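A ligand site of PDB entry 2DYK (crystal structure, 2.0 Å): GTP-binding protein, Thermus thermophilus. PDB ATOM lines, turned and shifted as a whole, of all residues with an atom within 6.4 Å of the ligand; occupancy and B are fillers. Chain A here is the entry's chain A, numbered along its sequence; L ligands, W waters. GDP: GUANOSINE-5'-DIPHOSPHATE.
O of Ser 15 sits close to NZ of Lys 40, 3.4 Å away. The backbone carbonyl oxygen (O) of Ser 16 sits close to the side-chain hydroxyl (OG) of Ser 143 (3.4 Å). N of Leu 17 lies within hydrogen-bond range of OG of Ser 143. The side-chain amino group of Lys 14 lies close to the backbone carbonyl oxygen of Gly 8. The backbone carbonyl oxygen (O) of Asp 119 is in hydrogen-bond range of a ring nitrogen (ND1) of His 145 (2.8 Å). The backbone carbonyl oxygen (O) of Asn 11 sits at hydrogen-bond distance from the side-chain amino group (NZ) of Lys 117, 2.8 Å away. O of Val 12 is in hydrogen-bond range of OG1 of Thr 116 (2.5 Å). The backbone carbonyl oxygen (O) of Thr 141 is in hydrogen-bond range of the backbone NH (N) of Lys 117 (3.2 Å).
The backbone NH of Ser 15 is in hydrogen-bond range of an oxygen (O3B) of the ligand (2.8 Å). O1A of the ligand sits at hydrogen-bond distance from OG of Ser 15. N of Ser 143 is in hydrogen-bond range of O6 of the ligand (2.7 Å). The backbone NH (N) of Lys 14 is in hydrogen-bond range of an oxygen (O2B) of the ligand (2.8 Å). NZ of Lys 14 is in salt-bridge range of O2B of the ligand (2.7 Å). A nitrogen (N2) of the ligand lies within hydrogen-bond range of the side-chain carboxylate of Asp 119 (2.7 Å). An oxygen (O1B) of the ligand sits at hydrogen-bond distance from the backbone NH (N) of Asn 11, at 2.8 Å. An oxygen (O1A) of the ligand sits at hydrogen-bond distance from the backbone NH of Ser 16 (3.0 Å). OG of Ser 16 lies within hydrogen-bond range of O1A of the ligand (2.9 Å). The backbone NH of Gly 13 lies within hydrogen-bond range of an oxygen (O3A) of the ligand, 2.9 Å away. The backbone NH (N) of Glu 144 lies within hydrogen-bond range of an oxygen (O6) of the ligand, at 3.1 Å. N of Val 12 is in hydrogen-bond range of O2B of the ligand (3.3 Å). O6 of the ligand sits close to OG of Ser 142 (3.5 Å).
Merely in contact with the ligand: Lys 117, Arg 90, Pro 10 and Arg 9. 14 residues have an atom within 4 Å of the ligand: Arg 9, Pro 10, Asn 11, Val 12, Gly 13, Lys 14, Ser 15, Ser 16, Arg 90, Lys 117, Asp 119, Ser 142, Ser 143 and Glu 144. The nearest printed residue that does not touch the ligand is Asp 55 (4.5 Å).
Water W3 bridges an oxygen (O1B) of the ligand (2.6 Å) and the side-chain amide oxygen (OD1) of Asn 11 (2.9 Å). Water W7 bridges the side-chain carboxylate of Asp 55 and an oxygen (O3B) of the ligand. Water W6 lies within hydrogen-bond range of O of Gly 13 (2.7 Å), N7 of the ligand (2.9 Å) and OG of Ser 143 (2.9 Å). Water W1 bridges O3B of the ligand and OG of Ser 15. Water W4 lies within hydrogen-bond range of the side-chain carboxylate (OE1) of Glu 144 (2.9 Å) and a nitrogen (N3) of the ligand (3.5 Å).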
ATOM      1  N   GLY A   8      26.256  33.010  21.080  1.00  0.00           N
ATOM      2  CA  GLY A   8      26.118  31.946  22.054  1.00  0.00           C
ATOM      3  C   GLY A   8      27.478  31.323  22.316  1.00  0.00           C
ATOM      4  O   GLY A   8      28.433  31.513  21.550  1.00  0.00           O
ATOM      5  N   ARG A   9      27.562  30.575  23.405  1.00  0.00           N
ATOM      6  CA  ARG A   9      28.810  29.938  23.757  1.00  0.00           C
ATOM      7  C   ARG A   9      29.178  28.803  22.807  1.00  0.00           C
ATOM      8  O   ARG A   9      28.367  28.349  22.003  1.00  0.00           O
ATOM      9  CB  ARG A   9      28.730  29.415  25.205  1.00  0.00           C
ATOM     10  CG  ARG A   9      27.855  28.195  25.389  1.00  0.00           C
ATOM     11  CD  ARG A   9      27.561  27.961  26.880  1.00  0.00           C
ATOM     12  NE  ARG A   9      26.556  26.915  27.077  1.00  0.00           N
ATOM     13  CZ  ARG A   9      26.794  25.602  27.010  1.00  0.00           C
ATOM     14  NH1 ARG A   9      28.011  25.144  26.748  1.00  0.00           N
ATOM     15  NH2 ARG A   9      25.813  24.742  27.238  1.00  0.00           N
ATOM     16  N   PRO A  10      30.439  28.333  22.878  1.00  0.00           N
ATOM     17  CA  PRO A  10      30.891  27.243  22.014  1.00  0.00           C
ATOM     18  C   PRO A  10      30.123  25.941  22.181  1.00  0.00           C
ATOM     19  O   PRO A  10      29.615  25.610  23.267  1.00  0.00           O
ATOM     20  CB  PRO A  10      32.373  27.099  22.406  1.00  0.00           C
ATOM     21  CG  PRO A  10      32.746  28.531  22.736  1.00  0.00           C
ATOM     22  CD  PRO A  10      31.570  28.966  23.576  1.00  0.00           C
ATOM     23  N   ASN A  11      30.018  25.213  21.087  1.00  0.00           N
ATOM     24  CA  ASN A  11      29.373  23.912  21.023  1.00  0.00           C
ATOM     25  C   ASN A  11      27.865  23.811  21.248  1.00  0.00           C
ATOM     26  O   ASN A  11      27.355  22.714  21.476  1.00  0.00           O
ATOM     27  CB  ASN A  11      30.089  22.937  21.953  1.00  0.00           C
ATOM     28  CG  ASN A  11      31.594  22.949  21.742  1.00  0.00           C
ATOM     29  OD1 ASN A  11      32.072  22.857  20.611  1.00  0.00           O
ATOM     30  ND2 ASN A  11      32.344  23.050  22.831  1.00  0.00           N
ATOM     31  N   VAL A  12      27.145  24.926  21.169  1.00  0.00           N
ATOM     32  CA  VAL A  12      25.695  24.848  21.363  1.00  0.00           C
ATOM     33  C   VAL A  12      25.005  24.580  20.021  1.00  0.00           C
ATOM     34  O   VAL A  12      23.801  24.387  19.976  1.00  0.00           O
ATOM     35  CB  VAL A  12      25.111  26.134  21.994  1.00  0.00           C
ATOM     36  CG1 VAL A  12      25.766  26.359  23.373  1.00  0.00           C
ATOM     37  CG2 VAL A  12      25.324  27.344  21.078  1.00  0.00           C
ATOM     38  N   GLY A  13      25.764  24.558  18.927  1.00  0.00           N
ATOM     39  CA  GLY A  13      25.181  24.256  17.632  1.00  0.00           C
ATOM     40  C   GLY A  13      24.963  25.419  16.699  1.00  0.00           C
ATOM     41  O   GLY A  13      24.137  25.321  15.784  1.00  0.00           O
ATOM     42  N   LYS A  14      25.696  26.499  16.889  1.00  0.00           N
ATOM     43  CA  LYS A  14      25.572  27.687  16.054  1.00  0.00           C
ATOM     44  C   LYS A  14      25.959  27.486  14.581  1.00  0.00           C
ATOM     45  O   LYS A  14      25.249  27.924  13.668  1.00  0.00           O
ATOM     46  CB  LYS A  14      26.371  28.841  16.667  1.00  0.00           C
ATOM     47  CG  LYS A  14      25.933  29.150  18.076  1.00  0.00           C
ATOM     48  CD  LYS A  14      26.634  30.366  18.717  1.00  0.00           C
ATOM     49  CE  LYS A  14      28.170  30.298  18.663  1.00  0.00           C
ATOM     50  NZ  LYS A  14      28.799  29.048  19.208  1.00  0.00           N
ATOM     51  N   SER A  15      27.091  26.825  14.332  1.00  0.00           N
ATOM     52  CA  SER A  15      27.524  26.643  12.952  1.00  0.00           C
ATOM     53  C   SER A  15      26.598  25.686  12.218  1.00  0.00           C
ATOM     54  O   SER A  15      26.361  25.844  11.027  1.00  0.00           O
ATOM     55  CB  SER A  15      28.969  26.137  12.896  1.00  0.00           C
ATOM     56  OG  SER A  15      29.094  24.902  13.573  1.00  0.00           O
ATOM     57  N   SER A  16      26.082  24.686  12.932  1.00  0.00           N
ATOM     58  CA  SER A  16      25.159  23.733  12.320  1.00  0.00           C
ATOM     59  C   SER A  16      23.864  24.458  11.961  1.00  0.00           C
ATOM     60  O   SER A  16      23.318  24.247  10.875  1.00  0.00           O
ATOM     61  CB  SER A  16      24.888  22.556  13.276  1.00  0.00           C
ATOM     62  OG  SER A  16      26.097  21.857  13.524  1.00  0.00           O
ATOM     63  N   LEU A  17      23.380  25.303  12.864  1.00  0.00           N
ATOM     64  CA  LEU A  17      22.173  26.081  12.621  1.00  0.00           C
ATOM     65  C   LEU A  17      22.402  27.051  11.438  1.00  0.00           C
ATOM     66  O   LEU A  17      21.544  27.192  10.553  1.00  0.00           O
ATOM     67  CB  LEU A  17      21.799  26.871  13.877  1.00  0.00           C
ATOM     68  CG  LEU A  17      20.604  27.824  13.715  1.00  0.00           C
ATOM     69  CD1 LEU A  17      19.349  27.000  13.431  1.00  0.00           C
ATOM     70  CD2 LEU A  17      20.437  28.687  14.957  1.00  0.00           C
ATOM     71  N   LYS A  40      31.392  33.891  10.249  1.00  0.00           N
ATOM     72  CA  LYS A  40      30.857  33.101   9.145  1.00  0.00           C
ATOM     73  C   LYS A  40      29.727  33.992   8.662  1.00  0.00           C
ATOM     74  O   LYS A  40      28.887  34.427   9.461  1.00  0.00           O
ATOM     75  CB  LYS A  40      30.318  31.756   9.616  1.00  0.00           C
ATOM     76  CG  LYS A  40      31.399  30.771  10.039  1.00  0.00           C
ATOM     77  CD  LYS A  40      30.787  29.565  10.734  1.00  0.00           C
ATOM     78  CE  LYS A  40      29.765  28.884   9.840  1.00  0.00           C
ATOM     79  NZ  LYS A  40      29.036  27.811  10.553  1.00  0.00           N
ATOM     80  N   ASP A  55      27.483  34.225  11.985  1.00  0.00           N
ATOM     81  CA  ASP A  55      27.722  33.369  13.146  1.00  0.00           C
ATOM     82  C   ASP A  55      28.985  33.919  13.793  1.00  0.00           C
ATOM     83  O   ASP A  55      30.009  34.092  13.131  1.00  0.00           O
ATOM     84  CB  ASP A  55      27.961  31.912  12.730  1.00  0.00           C
ATOM     85  CG  ASP A  55      28.343  31.009  13.918  1.00  0.00           C
ATOM     86  OD1 ASP A  55      28.140  31.434  15.081  1.00  0.00           O
ATOM     87  OD2 ASP A  55      28.830  29.887  13.699  1.00  0.00           O
ATOM     88  N   GLY A  57      30.484  32.443  16.541  1.00  0.00           N
ATOM     89  CA  GLY A  57      31.150  31.383  17.305  1.00  0.00           C
ATOM     90  C   GLY A  57      32.668  31.376  17.190  1.00  0.00           C
ATOM     91  O   GLY A  57      33.367  31.106  18.168  1.00  0.00           O
ATOM     92  N   ALA A  86      21.609  31.625  20.791  1.00  0.00           N
ATOM     93  CA  ALA A  86      21.618  30.183  20.815  1.00  0.00           C
ATOM     94  C   ALA A  86      22.035  29.592  22.169  1.00  0.00           C
ATOM     95  O   ALA A  86      23.150  29.855  22.668  1.00  0.00           O
ATOM     96  CB  ALA A  86      22.551  29.656  19.712  1.00  0.00           C
ATOM     97  N   ARG A  90      19.330  20.916  25.424  1.00  0.00           N
ATOM     98  CA  ARG A  90      19.402  19.699  26.233  1.00  0.00           C
ATOM     99  C   ARG A  90      20.236  19.908  27.491  1.00  0.00           C
ATOM    100  O   ARG A  90      19.806  19.563  28.603  1.00  0.00           O
ATOM    101  CB  ARG A  90      19.948  18.542  25.375  1.00  0.00           C
ATOM    102  CG  ARG A  90      19.047  18.180  24.181  1.00  0.00           C
ATOM    103  CD  ARG A  90      19.630  17.055  23.331  1.00  0.00           C
ATOM    104  NE  ARG A  90      21.010  17.349  22.923  1.00  0.00           N
ATOM    105  CZ  ARG A  90      21.789  16.507  22.245  1.00  0.00           C
ATOM    106  NH1 ARG A  90      21.331  15.311  21.891  1.00  0.00           N
ATOM    107  NH2 ARG A  90      23.020  16.857  21.929  1.00  0.00           N
ATOM    108  N   THR A 116      18.668  24.906  20.915  1.00  0.00           N
ATOM    109  CA  THR A 116      19.255  24.022  19.936  1.00  0.00           C
ATOM    110  C   THR A 116      19.263  22.579  20.366  1.00  0.00           C
ATOM    111  O   THR A 116      19.104  22.257  21.542  1.00  0.00           O
ATOM    112  CB  THR A 116      20.705  24.427  19.678  1.00  0.00           C
ATOM    113  OG1 THR A 116      21.442  24.305  20.908  1.00  0.00           O
ATOM    114  CG2 THR A 116      20.785  25.884  19.193  1.00  0.00           C
ATOM    115  N   LYS A 117      19.466  21.700  19.379  1.00  0.00           N
ATOM    116  CA  LYS A 117      19.538  20.261  19.582  1.00  0.00           C
ATOM    117  C   LYS A 117      18.244  19.685  20.167  1.00  0.00           C
ATOM    118  O   LYS A 117      18.292  18.663  20.863  1.00  0.00           O
ATOM    119  CB  LYS A 117      20.714  19.917  20.512  1.00  0.00           C
ATOM    120  CG  LYS A 117      22.059  20.505  20.056  1.00  0.00           C
ATOM    121  CD  LYS A 117      23.132  20.204  21.099  1.00  0.00           C
ATOM    122  CE  LYS A 117      24.478  20.794  20.704  1.00  0.00           C
ATOM    123  NZ  LYS A 117      25.478  20.598  21.767  1.00  0.00           N
ATOM    124  N   VAL A 118      17.113  20.339  19.935  1.00  0.00           N
ATOM    125  CA  VAL A 118      15.845  19.798  20.438  1.00  0.00           C
ATOM    126  C   VAL A 118      15.456  18.786  19.337  1.00  0.00           C
ATOM    127  O   VAL A 118      14.573  19.042  18.515  1.00  0.00           O
ATOM    128  CB  VAL A 118      14.766  20.910  20.552  1.00  0.00           C
ATOM    129  CG1 VAL A 118      13.499  20.349  21.181  1.00  0.00           C
ATOM    130  CG2 VAL A 118      15.285  22.071  21.383  1.00  0.00           C
ATOM    131  N   ASP A 119      16.124  17.637  19.353  1.00  0.00           N
ATOM    132  CA  ASP A 119      15.931  16.621  18.324  1.00  0.00           C
ATOM    133  C   ASP A 119      14.575  15.919  18.314  1.00  0.00           C
ATOM    134  O   ASP A 119      14.146  15.429  17.267  1.00  0.00           O
ATOM    135  CB  ASP A 119      17.035  15.570  18.413  1.00  0.00           C
ATOM    136  CG  ASP A 119      18.433  16.159  18.190  1.00  0.00           C
ATOM    137  OD1 ASP A 119      18.573  17.222  17.553  1.00  0.00           O
ATOM    138  OD2 ASP A 119      19.400  15.509  18.644  1.00  0.00           O
ATOM    139  N   THR A 141      14.752  24.273  18.113  1.00  0.00           N
ATOM    140  CA  THR A 141      15.256  23.874  16.815  1.00  0.00           C
ATOM    141  C   THR A 141      16.153  22.654  16.945  1.00  0.00           C
ATOM    142  O   THR A 141      16.555  22.268  18.051  1.00  0.00           O
ATOM    143  CB  THR A 141      16.071  24.985  16.116  1.00  0.00           C
ATOM    144  OG1 THR A 141      17.258  25.249  16.859  1.00  0.00           O
ATOM    145  CG2 THR A 141      15.244  26.245  15.979  1.00  0.00           C
ATOM    146  N   SER A 142      16.440  22.063  15.806  1.00  0.00           N
ATOM    147  CA  SER A 142      17.339  20.914  15.711  1.00  0.00           C
ATOM    148  C   SER A 142      17.951  20.993  14.331  1.00  0.00           C
ATOM    149  O   SER A 142      17.222  20.979  13.332  1.00  0.00           O
ATOM    150  CB  SER A 142      16.591  19.594  15.834  1.00  0.00           C
ATOM    151  OG  SER A 142      17.454  18.493  15.556  1.00  0.00           O
ATOM    152  N   SER A 143      19.272  21.112  14.247  1.00  0.00           N
ATOM    153  CA  SER A 143      19.915  21.144  12.939  1.00  0.00           C
ATOM    154  C   SER A 143      20.086  19.717  12.460  1.00  0.00           C
ATOM    155  O   SER A 143      20.103  19.460  11.264  1.00  0.00           O
ATOM    156  CB  SER A 143      21.283  21.839  13.001  1.00  0.00           C
ATOM    157  OG  SER A 143      21.128  23.199  13.286  1.00  0.00           O
ATOM    158  N   GLU A 144      20.197  18.786  13.391  1.00  0.00           N
ATOM    159  CA  GLU A 144      20.343  17.372  13.058  1.00  0.00           C
ATOM    160  C   GLU A 144      19.073  16.862  12.361  1.00  0.00           C
ATOM    161  O   GLU A 144      19.152  16.130  11.368  1.00  0.00           O
ATOM    162  CB  GLU A 144      20.602  16.538  14.321  1.00  0.00           C
ATOM    163  CG  GLU A 144      21.170  15.153  14.066  1.00  0.00           C
ATOM    164  CD  GLU A 144      22.580  15.203  13.504  1.00  0.00           C
ATOM    165  OE1 GLU A 144      23.461  15.847  14.127  1.00  0.00           O
ATOM    166  OE2 GLU A 144      22.822  14.592  12.429  1.00  0.00           O
ATOM    167  N   HIS A 145      17.906  17.248  12.865  1.00  0.00           N
ATOM    168  CA  HIS A 145      16.627  16.809  12.284  1.00  0.00           C
ATOM    169  C   HIS A 145      15.880  17.880  11.502  1.00  0.00           C
ATOM    170  O   HIS A 145      14.727  17.653  11.091  1.00  0.00           O
ATOM    171  CB  HIS A 145      15.699  16.286  13.380  1.00  0.00           C
ATOM    172  CG  HIS A 145      16.146  14.995  13.976  1.00  0.00           C
ATOM    173  ND1 HIS A 145      15.492  14.398  15.030  1.00  0.00           N
ATOM    174  CD2 HIS A 145      17.190  14.190  13.675  1.00  0.00           C
ATOM    175  CE1 HIS A 145      16.114  13.283  15.367  1.00  0.00           C
ATOM    176  NE2 HIS A 145      17.152  13.134  14.552  1.00  0.00           N
HETATM  177  PB  GDP L   1      29.150  25.779  17.675  1.00  0.00           P
HETATM  178  O1B GDP L   1      30.426  25.473  18.363  1.00  0.00           O
HETATM  179  O2B GDP L   1      27.968  26.553  18.452  1.00  0.00           O
HETATM  180  O3B GDP L   1      29.096  26.098  16.092  1.00  0.00           O
HETATM  181  O3A GDP L   1      28.399  24.354  17.664  1.00  0.00           O
HETATM  182  PA  GDP L   1      28.327  23.268  16.474  1.00  0.00           P
HETATM  183  O1A GDP L   1      27.469  23.675  15.349  1.00  0.00           O
HETATM  184  O2A GDP L   1      29.829  22.930  15.995  1.00  0.00           O
HETATM  185  O5' GDP L   1      27.787  21.917  17.159  1.00  0.00           O
HETATM  186  C5' GDP L   1      28.500  21.338  18.250  1.00  0.00           C
HETATM  187  C4' GDP L   1      28.208  19.837  18.361  1.00  0.00           C
HETATM  188  O4' GDP L   1      26.777  19.668  18.450  1.00  0.00           O
HETATM  189  C3' GDP L   1      28.640  19.165  17.047  1.00  0.00           C
HETATM  190  O3' GDP L   1      28.932  17.792  17.288  1.00  0.00           O
HETATM  191  C2' GDP L   1      27.376  19.335  16.210  1.00  0.00           C
HETATM  192  O2' GDP L   1      27.333  18.340  15.188  1.00  0.00           O
HETATM  193  C1' GDP L   1      26.327  18.987  17.264  1.00  0.00           C
HETATM  194  N9  GDP L   1      24.981  19.459  16.859  1.00  0.00           N
HETATM  195  C8  GDP L   1      24.703  20.617  16.262  1.00  0.00           C
HETATM  196  N7  GDP L   1      23.383  20.724  16.115  1.00  0.00           N
HETATM  197  C5  GDP L   1      22.819  19.630  16.613  1.00  0.00           C
HETATM  198  C6  GDP L   1      21.499  19.206  16.721  1.00  0.00           C
HETATM  199  O6  GDP L   1      20.564  19.874  16.304  1.00  0.00           O
HETATM  200  N1  GDP L   1      21.242  17.967  17.339  1.00  0.00           N
HETATM  201  C2  GDP L   1      22.311  17.206  17.811  1.00  0.00           C
HETATM  202  N2  GDP L   1      22.079  16.054  18.449  1.00  0.00           N
HETATM  203  N3  GDP L   1      23.567  17.643  17.671  1.00  0.00           N
HETATM  204  C4  GDP L   1      23.839  18.823  17.089  1.00  0.00           C
HETATM  205  O   HOH W   1      31.953  25.173  15.406  1.00  0.00           O
HETATM  206  O   HOH W   2      32.378  27.174  18.350  1.00  0.00           O
HETATM  207  O   HOH W   3      32.223  23.604  17.843  1.00  0.00           O
HETATM  208  O   HOH W   4      25.289  14.981  16.231  1.00  0.00           O
HETATM  209  O   HOH W   5      19.400  23.102  16.805  1.00  0.00           O
HETATM  210  O   HOH W   6      22.246  23.394  15.991  1.00  0.00           O
HETATM  211  O   HOH W   7      29.942  28.723  15.609  1.00  0.00           O
